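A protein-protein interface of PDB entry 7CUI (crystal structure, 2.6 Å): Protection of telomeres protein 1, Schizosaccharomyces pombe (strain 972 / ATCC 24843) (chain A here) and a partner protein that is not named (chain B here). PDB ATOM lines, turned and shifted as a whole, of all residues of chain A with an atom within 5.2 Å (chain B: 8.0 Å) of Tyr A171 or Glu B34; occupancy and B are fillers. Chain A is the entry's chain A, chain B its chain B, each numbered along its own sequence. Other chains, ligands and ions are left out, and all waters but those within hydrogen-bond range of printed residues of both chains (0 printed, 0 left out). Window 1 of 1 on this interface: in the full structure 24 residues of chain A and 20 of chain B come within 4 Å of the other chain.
OH of Tyr A171 lies within hydrogen-bond range of O of Glu B34. The backbone carbonyl oxygen (O) of Ile A172 lies within hydrogen-bond range of the side-chain amide nitrogen (NE2) of Gln B41 (2.9 Å). NH2 of Arg A190 is in salt-bridge range of OE2 of Glu B34, 3.0 Å away. The backbone carbonyl oxygen (O) of Cys B35 is in hydrogen-bond range of the guanidinium group (NE) of Arg A192. O of Ile A175 lies close to OE2 of Glu B33 (3.4 Å).
The backbone NH (N) of Ile A97 lies within hydrogen-bond range of the backbone carbonyl oxygen (O) of Trp A191 (2.9 Å). O of Arg A192 lies within hydrogen-bond range of N of Lys A169 (2.8 Å). The backbone carbonyl oxygen (O) of Tyr A171 sits at hydrogen-bond distance from the backbone NH (N) of Arg A190 (2.8 Å). The side-chain amide oxygen (OD1) of Asn B26 sits close to the side-chain carboxylate (OE2) of Glu B34. The side-chain hydroxyl (OG) of Ser B31 lies within hydrogen-bond range of the side-chain carboxylate (OE1) of Glu B34, 3.0 Å away. The backbone carbonyl oxygen (O) of Ile B37 is in hydrogen-bond range of the side-chain amide nitrogen (NE2) of Gln B42 (3.2 Å).
Pro A48 touches Leu B45 (CB to CG, 3.9 Å). Ile A97 touches Cys B35. Lys A169 touches Ile B37 (CE to CD1, 3.8 Å). OH of Tyr A171 touches CA of Cys B35 (3.4 Å). Tyr A171 touches Ile B36 (CE2 to O, 3.7 Å). CD2 of Tyr A171 touches CG1 of Ile B37, 3.8 Å away. Tyr A171 touches Gln B41 (CB to OE1, 3.3 Å). Pro A173 touches Glu B34. O of Ile B36 touches CB of Pro A173 (3.5 Å). Ile B37 touches Arg A192.
Tyr A171 touches five residues of chain B. Glu B34 touches just these residues of chain A: Tyr A171, Pro A173 and Arg A190. Printed residues of chain B within 4 Å of Ile A97: Asn B26, Leu B30 and Cys B35. Of the printed residues of chain A, Gln B41 touches Pro A48, Tyr A171 and Ile A172. The nearest residue of chain B that does not touch Tyr A171 is Pro B38 (4.4 Å).
Hydrophobic or aromatic side chains of chain A within 4 Å of the printed part of chain B: Pro A48, Ile A97, Tyr A171 and Pro A173. Along chain A the printed residues that touch a printed residue of chain B span positions 48 to 192. Printed residues of chain B that touch a printed residue of chain A: Asn B26, Leu B30, Glu B33, Glu B34, Cys B35, Ile B36, Ile B37, Pro B38, Gln B41 and Leu B45. Among the printed residues, 20 pairs touch across the chains. Among the printed residues, Asp or Glu carboxylates within 4 Å of a Lys or Arg side-chain nitrogen of the other chain: Arg A190 with Glu B34.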
ATOM      1  N   PRO A  48      -3.931   0.392 -16.021  1.00  0.00           N
ATOM      2  CA  PRO A  48      -4.892   1.142 -15.210  1.00  0.00           C
ATOM      3  C   PRO A  48      -5.495   0.290 -14.093  1.00  0.00           C
ATOM      4  O   PRO A  48      -5.850  -0.868 -14.308  1.00  0.00           O
ATOM      5  CB  PRO A  48      -5.960   1.595 -16.215  1.00  0.00           C
ATOM      6  CG  PRO A  48      -5.876   0.580 -17.331  1.00  0.00           C
ATOM      7  CD  PRO A  48      -4.424   0.149 -17.387  1.00  0.00           C
ATOM      8  N   ILE A  97      -7.001  13.786  -8.170  1.00  0.00           N
ATOM      9  CA  ILE A  97      -7.510  14.843  -9.028  1.00  0.00           C
ATOM     10  C   ILE A  97      -9.017  14.674  -9.200  1.00  0.00           C
ATOM     11  O   ILE A  97      -9.491  13.589  -9.535  1.00  0.00           O
ATOM     12  CB  ILE A  97      -6.788  14.834 -10.391  1.00  0.00           C
ATOM     13  CG1 ILE A  97      -5.298  15.156 -10.255  1.00  0.00           C
ATOM     14  CG2 ILE A  97      -7.473  15.771 -11.376  1.00  0.00           C
ATOM     15  CD1 ILE A  97      -4.475  14.766 -11.467  1.00  0.00           C
ATOM     16  N   LYS A 169      -9.236   6.199  -9.774  1.00  0.00           N
ATOM     17  CA  LYS A 169      -8.785   5.494 -10.960  1.00  0.00           C
ATOM     18  C   LYS A 169      -7.355   5.924 -11.276  1.00  0.00           C
ATOM     19  O   LYS A 169      -7.073   7.110 -11.423  1.00  0.00           O
ATOM     20  CB  LYS A 169      -9.763   5.661 -12.128  1.00  0.00           C
ATOM     21  CG  LYS A 169     -10.222   7.079 -12.441  1.00  0.00           C
ATOM     22  CD  LYS A 169     -11.414   7.106 -13.375  1.00  0.00           C
ATOM     23  CE  LYS A 169     -12.097   8.456 -13.414  1.00  0.00           C
ATOM     24  NZ  LYS A 169     -13.325   8.430 -14.244  1.00  0.00           N
ATOM     25  N   GLU A 170      -6.464   4.932 -11.342  1.00  0.00           N
ATOM     26  CA  GLU A 170      -5.046   5.123 -11.597  1.00  0.00           C
ATOM     27  C   GLU A 170      -4.809   4.991 -13.096  1.00  0.00           C
ATOM     28  O   GLU A 170      -5.362   4.096 -13.731  1.00  0.00           O
ATOM     29  CB  GLU A 170      -4.265   4.051 -10.837  1.00  0.00           C
ATOM     30  CG  GLU A 170      -2.763   4.266 -10.802  1.00  0.00           C
ATOM     31  CD  GLU A 170      -2.055   3.302  -9.863  1.00  0.00           C
ATOM     32  OE1 GLU A 170      -2.690   2.320  -9.440  1.00  0.00           O
ATOM     33  OE2 GLU A 170      -0.877   3.539  -9.547  1.00  0.00           O
ATOM     34  N   TYR A 171      -3.980   5.884 -13.647  1.00  0.00           N
ATOM     35  CA  TYR A 171      -3.767   5.958 -15.084  1.00  0.00           C
ATOM     36  C   TYR A 171      -2.495   6.748 -15.371  1.00  0.00           C
ATOM     37  O   TYR A 171      -1.952   7.398 -14.484  1.00  0.00           O
ATOM     38  CB  TYR A 171      -4.957   6.637 -15.769  1.00  0.00           C
ATOM     39  CG  TYR A 171      -5.103   8.101 -15.434  1.00  0.00           C
ATOM     40  CD1 TYR A 171      -5.662   8.506 -14.233  1.00  0.00           C
ATOM     41  CD2 TYR A 171      -4.665   9.085 -16.310  1.00  0.00           C
ATOM     42  CE1 TYR A 171      -5.782   9.847 -13.909  1.00  0.00           C
ATOM     43  CE2 TYR A 171      -4.783  10.431 -16.005  1.00  0.00           C
ATOM     44  CZ  TYR A 171      -5.348  10.814 -14.800  1.00  0.00           C
ATOM     45  OH  TYR A 171      -5.472  12.136 -14.487  1.00  0.00           O
ATOM     46  N   ILE A 172      -2.046   6.697 -16.629  1.00  0.00           N
ATOM     47  CA  ILE A 172      -0.852   7.402 -17.067  1.00  0.00           C
ATOM     48  C   ILE A 172      -1.233   8.288 -18.249  1.00  0.00           C
ATOM     49  O   ILE A 172      -1.473   7.771 -19.341  1.00  0.00           O
ATOM     50  CB  ILE A 172       0.252   6.399 -17.466  1.00  0.00           C
ATOM     51  CG1 ILE A 172       0.555   5.393 -16.351  1.00  0.00           C
ATOM     52  CG2 ILE A 172       1.507   7.127 -17.932  1.00  0.00           C
ATOM     53  CD1 ILE A 172       1.151   4.086 -16.837  1.00  0.00           C
ATOM     54  N   PRO A 173      -1.293   9.635 -18.102  1.00  0.00           N
ATOM     55  CA  PRO A 173      -1.702  10.487 -19.217  1.00  0.00           C
ATOM     56  C   PRO A 173      -0.537  10.747 -20.167  1.00  0.00           C
ATOM     57  O   PRO A 173       0.623  10.539 -19.812  1.00  0.00           O
ATOM     58  CB  PRO A 173      -2.107  11.789 -18.514  1.00  0.00           C
ATOM     59  CG  PRO A 173      -1.170  11.858 -17.327  1.00  0.00           C
ATOM     60  CD  PRO A 173      -0.966  10.416 -16.896  1.00  0.00           C
ATOM     61  N   ILE A 175       1.636  13.307 -21.594  1.00  0.00           N
ATOM     62  CA  ILE A 175       2.142  14.664 -21.445  1.00  0.00           C
ATOM     63  C   ILE A 175       3.324  14.850 -22.406  1.00  0.00           C
ATOM     64  O   ILE A 175       3.132  15.533 -23.433  1.00  0.00           O
ATOM     65  CB  ILE A 175       2.534  14.975 -19.982  1.00  0.00           C
ATOM     66  CG1 ILE A 175       3.692  14.094 -19.504  1.00  0.00           C
ATOM     67  CG2 ILE A 175       1.328  14.884 -19.055  1.00  0.00           C
ATOM     68  CD1 ILE A 175       4.777  14.840 -18.757  1.00  0.00           C
ATOM     69  N   GLN A 188       4.919   9.147 -13.333  1.00  0.00           N
ATOM     70  CA  GLN A 188       4.122   9.452 -14.511  1.00  0.00           C
ATOM     71  C   GLN A 188       2.672   9.022 -14.303  1.00  0.00           C
ATOM     72  O   GLN A 188       1.822   9.288 -15.150  1.00  0.00           O
ATOM     73  CB  GLN A 188       4.725   8.815 -15.765  1.00  0.00           C
ATOM     74  CG  GLN A 188       5.805   9.663 -16.428  1.00  0.00           C
ATOM     75  CD  GLN A 188       7.165   9.491 -15.797  1.00  0.00           C
ATOM     76  OE1 GLN A 188       7.432   8.508 -15.115  1.00  0.00           O
ATOM     77  NE2 GLN A 188       8.043  10.453 -16.025  1.00  0.00           N
ATOM     78  N   LYS A 189       2.393   8.368 -13.172  1.00  0.00           N
ATOM     79  CA  LYS A 189       1.030   7.969 -12.860  1.00  0.00           C
ATOM     80  C   LYS A 189       0.280   9.140 -12.228  1.00  0.00           C
ATOM     81  O   LYS A 189       0.866   9.950 -11.513  1.00  0.00           O
ATOM     82  CB  LYS A 189       1.018   6.728 -11.962  1.00  0.00           C
ATOM     83  CG  LYS A 189       1.401   5.426 -12.653  1.00  0.00           C
ATOM     84  CD  LYS A 189       1.307   4.218 -11.744  1.00  0.00           C
ATOM     85  CE  LYS A 189       1.231   2.896 -12.480  1.00  0.00           C
ATOM     86  NZ  LYS A 189      -0.106   2.662 -13.078  1.00  0.00           N
ATOM     87  N   ARG A 190      -1.022   9.213 -12.527  1.00  0.00           N
ATOM     88  CA  ARG A 190      -1.949  10.153 -11.916  1.00  0.00           C
ATOM     89  C   ARG A 190      -3.119   9.368 -11.325  1.00  0.00           C
ATOM     90  O   ARG A 190      -3.431   8.272 -11.788  1.00  0.00           O
ATOM     91  CB  ARG A 190      -2.468  11.144 -12.965  1.00  0.00           C
ATOM     92  CG  ARG A 190      -1.786  12.505 -12.978  1.00  0.00           C
ATOM     93  CD  ARG A 190      -0.276  12.455 -12.860  1.00  0.00           C
ATOM     94  NE  ARG A 190       0.389  13.717 -13.136  1.00  0.00           N
ATOM     95  CZ  ARG A 190       1.707  13.866 -13.204  1.00  0.00           C
ATOM     96  NH1 ARG A 190       2.504  12.826 -13.015  1.00  0.00           N
ATOM     97  NH2 ARG A 190       2.224  15.053 -13.467  1.00  0.00           N
ATOM     98  N   TRP A 191      -3.761   9.943 -10.302  1.00  0.00           N
ATOM     99  CA  TRP A 191      -4.960   9.367  -9.712  1.00  0.00           C
ATOM    100  C   TRP A 191      -6.122  10.345  -9.831  1.00  0.00           C
ATOM    101  O   TRP A 191      -5.955  11.545  -9.628  1.00  0.00           O
ATOM    102  CB  TRP A 191      -4.727   8.988  -8.248  1.00  0.00           C
ATOM    103  CG  TRP A 191      -3.708   7.908  -8.081  1.00  0.00           C
ATOM    104  CD1 TRP A 191      -3.937   6.567  -7.972  1.00  0.00           C
ATOM    105  CD2 TRP A 191      -2.283   8.084  -8.031  1.00  0.00           C
ATOM    106  NE1 TRP A 191      -2.750   5.897  -7.850  1.00  0.00           N
ATOM    107  CE2 TRP A 191      -1.718   6.800  -7.879  1.00  0.00           C
ATOM    108  CE3 TRP A 191      -1.433   9.195  -8.094  1.00  0.00           C
ATOM    109  CZ2 TRP A 191      -0.340   6.603  -7.789  1.00  0.00           C
ATOM    110  CZ3 TRP A 191      -0.072   9.000  -8.007  1.00  0.00           C
ATOM    111  CH2 TRP A 191       0.466   7.719  -7.855  1.00  0.00           C
ATOM    112  N   ARG A 192      -7.308   9.799 -10.116  1.00  0.00           N
ATOM    113  CA  ARG A 192      -8.499  10.601 -10.328  1.00  0.00           C
ATOM    114  C   ARG A 192      -9.642  10.073  -9.465  1.00  0.00           C
ATOM    115  O   ARG A 192     -10.004   8.903  -9.562  1.00  0.00           O
ATOM    116  CB  ARG A 192      -8.867  10.576 -11.812  1.00  0.00           C
ATOM    117  CG  ARG A 192      -8.398  11.801 -12.581  1.00  0.00           C
ATOM    118  CD  ARG A 192      -9.604  12.554 -13.094  1.00  0.00           C
ATOM    119  NE  ARG A 192      -9.738  12.426 -14.535  1.00  0.00           N
ATOM    120  CZ  ARG A 192     -10.889  12.363 -15.197  1.00  0.00           C
ATOM    121  NH1 ARG A 192     -12.042  12.378 -14.550  1.00  0.00           N
ATOM    122  NH2 ARG A 192     -10.879  12.270 -16.514  1.00  0.00           N
ATOM    123  N   LYS B  25       3.910  16.672  -7.239  1.00  0.00           N
ATOM    124  CA  LYS B  25       3.934  17.714  -8.254  1.00  0.00           C
ATOM    125  C   LYS B  25       2.612  18.481  -8.253  1.00  0.00           C
ATOM    126  O   LYS B  25       2.605  19.696  -8.444  1.00  0.00           O
ATOM    127  CB  LYS B  25       4.221  17.122  -9.639  1.00  0.00           C
ATOM    128  CG  LYS B  25       5.380  16.135  -9.713  1.00  0.00           C
ATOM    129  CD  LYS B  25       5.881  15.920 -11.127  1.00  0.00           C
ATOM    130  CE  LYS B  25       6.560  14.583 -11.333  1.00  0.00           C
ATOM    131  NZ  LYS B  25       7.000  14.410 -12.737  1.00  0.00           N
ATOM    132  N   ASN B  26       1.508  17.762  -8.006  1.00  0.00           N
ATOM    133  CA  ASN B  26       0.161  18.291  -8.162  1.00  0.00           C
ATOM    134  C   ASN B  26      -0.149  19.339  -7.094  1.00  0.00           C
ATOM    135  O   ASN B  26      -1.099  20.105  -7.245  1.00  0.00           O
ATOM    136  CB  ASN B  26      -0.890  17.179  -8.199  1.00  0.00           C
ATOM    137  CG  ASN B  26      -0.832  16.361  -9.471  1.00  0.00           C
ATOM    138  OD1 ASN B  26      -0.455  16.866 -10.527  1.00  0.00           O
ATOM    139  ND2 ASN B  26      -1.205  15.095  -9.382  1.00  0.00           N
ATOM    140  N   MET B  27       0.669  19.377  -6.034  1.00  0.00           N
ATOM    141  CA  MET B  27       0.482  20.317  -4.939  1.00  0.00           C
ATOM    142  C   MET B  27       1.175  21.645  -5.246  1.00  0.00           C
ATOM    143  O   MET B  27       1.166  22.546  -4.408  1.00  0.00           O
ATOM    144  CB  MET B  27       0.998  19.723  -3.622  1.00  0.00           C
ATOM    145  CG  MET B  27       0.092  18.673  -3.013  1.00  0.00           C
ATOM    146  SD  MET B  27      -1.727  19.348  -2.712  1.00  0.00           S
ATOM    147  CE  MET B  27      -2.990  18.489  -3.948  1.00  0.00           C
ATOM    148  N   SER B  29       1.513  22.476  -9.121  1.00  0.00           N
ATOM    149  CA  SER B  29       1.075  22.752 -10.483  1.00  0.00           C
ATOM    150  C   SER B  29       0.117  21.663 -10.962  1.00  0.00           C
ATOM    151  O   SER B  29       0.229  20.509 -10.555  1.00  0.00           O
ATOM    152  CB  SER B  29       2.257  22.881 -11.411  1.00  0.00           C
ATOM    153  OG  SER B  29       3.026  21.686 -11.425  1.00  0.00           O
ATOM    154  N   LEU B  30      -0.824  22.040 -11.834  1.00  0.00           N
ATOM    155  CA  LEU B  30      -1.788  21.096 -12.377  1.00  0.00           C
ATOM    156  C   LEU B  30      -2.352  21.630 -13.690  1.00  0.00           C
ATOM    157  O   LEU B  30      -2.806  22.772 -13.760  1.00  0.00           O
ATOM    158  CB  LEU B  30      -2.896  20.863 -11.342  1.00  0.00           C
ATOM    159  CG  LEU B  30      -4.041  19.933 -11.754  1.00  0.00           C
ATOM    160  CD1 LEU B  30      -3.557  18.511 -12.000  1.00  0.00           C
ATOM    161  CD2 LEU B  30      -5.136  19.940 -10.700  1.00  0.00           C
ATOM    162  N   SER B  31      -2.332  20.774 -14.718  1.00  0.00           N
ATOM    163  CA  SER B  31      -2.751  21.146 -16.060  1.00  0.00           C
ATOM    164  C   SER B  31      -3.820  20.181 -16.568  1.00  0.00           C
ATOM    165  O   SER B  31      -3.976  19.086 -16.035  1.00  0.00           O
ATOM    166  CB  SER B  31      -1.570  21.189 -16.989  1.00  0.00           C
ATOM    167  OG  SER B  31      -1.047  19.885 -17.179  1.00  0.00           O
ATOM    168  N   ILE B  32      -4.538  20.595 -17.617  1.00  0.00           N
ATOM    169  CA  ILE B  32      -5.614  19.805 -18.195  1.00  0.00           C
ATOM    170  C   ILE B  32      -5.053  18.522 -18.812  1.00  0.00           C
ATOM    171  O   ILE B  32      -5.710  17.485 -18.758  1.00  0.00           O
ATOM    172  CB  ILE B  32      -6.458  20.653 -19.173  1.00  0.00           C
ATOM    173  CG1 ILE B  32      -7.162  21.796 -18.430  1.00  0.00           C
ATOM    174  CG2 ILE B  32      -7.445  19.787 -19.947  1.00  0.00           C
ATOM    175  CD1 ILE B  32      -7.898  22.784 -19.312  1.00  0.00           C
ATOM    176  N   GLU B  33      -3.833  18.592 -19.363  1.00  0.00           N
ATOM    177  CA  GLU B  33      -3.132  17.436 -19.907  1.00  0.00           C
ATOM    178  C   GLU B  33      -3.240  16.251 -18.948  1.00  0.00           C
ATOM    179  O   GLU B  33      -3.652  15.163 -19.350  1.00  0.00           O
ATOM    180  CB  GLU B  33      -1.646  17.749 -20.094  1.00  0.00           C
ATOM    181  CG  GLU B  33      -1.250  18.114 -21.508  1.00  0.00           C
ATOM    182  CD  GLU B  33       0.250  18.292 -21.688  1.00  0.00           C
ATOM    183  OE1 GLU B  33       0.911  18.770 -20.739  1.00  0.00           O
ATOM    184  OE2 GLU B  33       0.756  17.943 -22.774  1.00  0.00           O
ATOM    185  N   GLU B  34      -2.875  16.492 -17.681  1.00  0.00           N
ATOM    186  CA  GLU B  34      -2.650  15.452 -16.686  1.00  0.00           C
ATOM    187  C   GLU B  34      -3.963  14.777 -16.298  1.00  0.00           C
ATOM    188  O   GLU B  34      -3.945  13.683 -15.737  1.00  0.00           O
ATOM    189  CB  GLU B  34      -2.012  16.037 -15.425  1.00  0.00           C
ATOM    190  CG  GLU B  34      -0.700  16.759 -15.665  1.00  0.00           C
ATOM    191  CD  GLU B  34      -0.234  17.561 -14.464  1.00  0.00           C
ATOM    192  OE1 GLU B  34      -0.060  18.789 -14.604  1.00  0.00           O
ATOM    193  OE2 GLU B  34      -0.052  16.956 -13.388  1.00  0.00           O
ATOM    194  N   CYS B  35      -5.086  15.446 -16.588  1.00  0.00           N
ATOM    195  CA  CYS B  35      -6.399  15.017 -16.136  1.00  0.00           C
ATOM    196  C   CYS B  35      -7.042  14.076 -17.155  1.00  0.00           C
ATOM    197  O   CYS B  35      -7.980  13.353 -16.824  1.00  0.00           O
ATOM    198  CB  CYS B  35      -7.315  16.215 -15.911  1.00  0.00           C
ATOM    199  SG  CYS B  35      -6.717  17.370 -14.651  1.00  0.00           S
ATOM    200  N   ILE B  36      -6.533  14.092 -18.392  1.00  0.00           N
ATOM    201  CA  ILE B  36      -7.132  13.338 -19.484  1.00  0.00           C
ATOM    202  C   ILE B  36      -6.643  11.892 -19.422  1.00  0.00           C
ATOM    203  O   ILE B  36      -5.443  11.635 -19.480  1.00  0.00           O
ATOM    204  CB  ILE B  36      -6.822  13.993 -20.847  1.00  0.00           C
ATOM    205  CG1 ILE B  36      -7.408  15.405 -20.935  1.00  0.00           C
ATOM    206  CG2 ILE B  36      -7.279  13.105 -22.001  1.00  0.00           C
ATOM    207  CD1 ILE B  36      -6.789  16.268 -22.012  1.00  0.00           C
ATOM    208  N   ILE B  37      -7.593  10.958 -19.309  1.00  0.00           N
ATOM    209  CA  ILE B  37      -7.281   9.539 -19.332  1.00  0.00           C
ATOM    210  C   ILE B  37      -7.291   9.087 -20.789  1.00  0.00           C
ATOM    211  O   ILE B  37      -8.319   9.210 -21.453  1.00  0.00           O
ATOM    212  CB  ILE B  37      -8.298   8.738 -18.491  1.00  0.00           C
ATOM    213  CG1 ILE B  37      -8.344   9.227 -17.039  1.00  0.00           C
ATOM    214  CG2 ILE B  37      -8.008   7.246 -18.572  1.00  0.00           C
ATOM    215  CD1 ILE B  37      -9.587   8.815 -16.280  1.00  0.00           C
ATOM    216  N   PRO B  38      -6.169   8.554 -21.335  1.00  0.00           N
ATOM    217  CA  PRO B  38      -6.147   8.067 -22.718  1.00  0.00           C
ATOM    218  C   PRO B  38      -7.271   7.068 -22.982  1.00  0.00           C
ATOM    219  O   PRO B  38      -7.653   6.305 -22.097  1.00  0.00           O
ATOM    220  CB  PRO B  38      -4.773   7.396 -22.848  1.00  0.00           C
ATOM    221  CG  PRO B  38      -3.925   8.097 -21.810  1.00  0.00           C
ATOM    222  CD  PRO B  38      -4.868   8.400 -20.664  1.00  0.00           C
ATOM    223  N   GLN B  41      -6.928   3.384 -22.050  1.00  0.00           N
ATOM    224  CA  GLN B  41      -6.910   3.110 -20.623  1.00  0.00           C
ATOM    225  C   GLN B  41      -8.309   3.294 -20.047  1.00  0.00           C
ATOM    226  O   GLN B  41      -8.678   2.616 -19.091  1.00  0.00           O
ATOM    227  CB  GLN B  41      -5.915   4.018 -19.903  1.00  0.00           C
ATOM    228  CG  GLN B  41      -4.465   3.734 -20.260  1.00  0.00           C
ATOM    229  CD  GLN B  41      -3.533   4.662 -19.523  1.00  0.00           C
ATOM    230  OE1 GLN B  41      -3.687   4.902 -18.328  1.00  0.00           O
ATOM    231  NE2 GLN B  41      -2.558   5.194 -20.239  1.00  0.00           N
ATOM    232  N   GLN B  42      -9.076   4.216 -20.642  1.00  0.00           N
ATOM    233  CA  GLN B  42     -10.447   4.478 -20.235  1.00  0.00           C
ATOM    234  C   GLN B  42     -11.299   3.242 -20.515  1.00  0.00           C
ATOM    235  O   GLN B  42     -12.148   2.872 -19.707  1.00  0.00           O
ATOM    236  CB  GLN B  42     -10.992   5.715 -20.953  1.00  0.00           C
ATOM    237  CG  GLN B  42     -12.042   6.475 -20.154  1.00  0.00           C
ATOM    238  CD  GLN B  42     -12.379   7.801 -20.794  1.00  0.00           C
ATOM    239  OE1 GLN B  42     -13.470   7.995 -21.326  1.00  0.00           O
ATOM    240  NE2 GLN B  42     -11.434   8.729 -20.756  1.00  0.00           N
ATOM    241  N   LEU B  45     -10.790   0.478 -17.890  1.00  0.00           N
ATOM    242  CA  LEU B  45     -11.474   0.793 -16.645  1.00  0.00           C
ATOM    243  C   LEU B  45     -12.981   0.585 -16.795  1.00  0.00           C
ATOM    244  O   LEU B  45     -13.623   0.077 -15.880  1.00  0.00           O
ATOM    245  CB  LEU B  45     -11.144   2.232 -16.231  1.00  0.00           C
ATOM    246  CG  LEU B  45      -9.710   2.467 -15.754  1.00  0.00           C
ATOM    247  CD1 LEU B  45      -9.313   3.923 -15.927  1.00  0.00           C
ATOM    248  CD2 LEU B  45      -9.537   2.040 -14.304  1.00  0.00           C
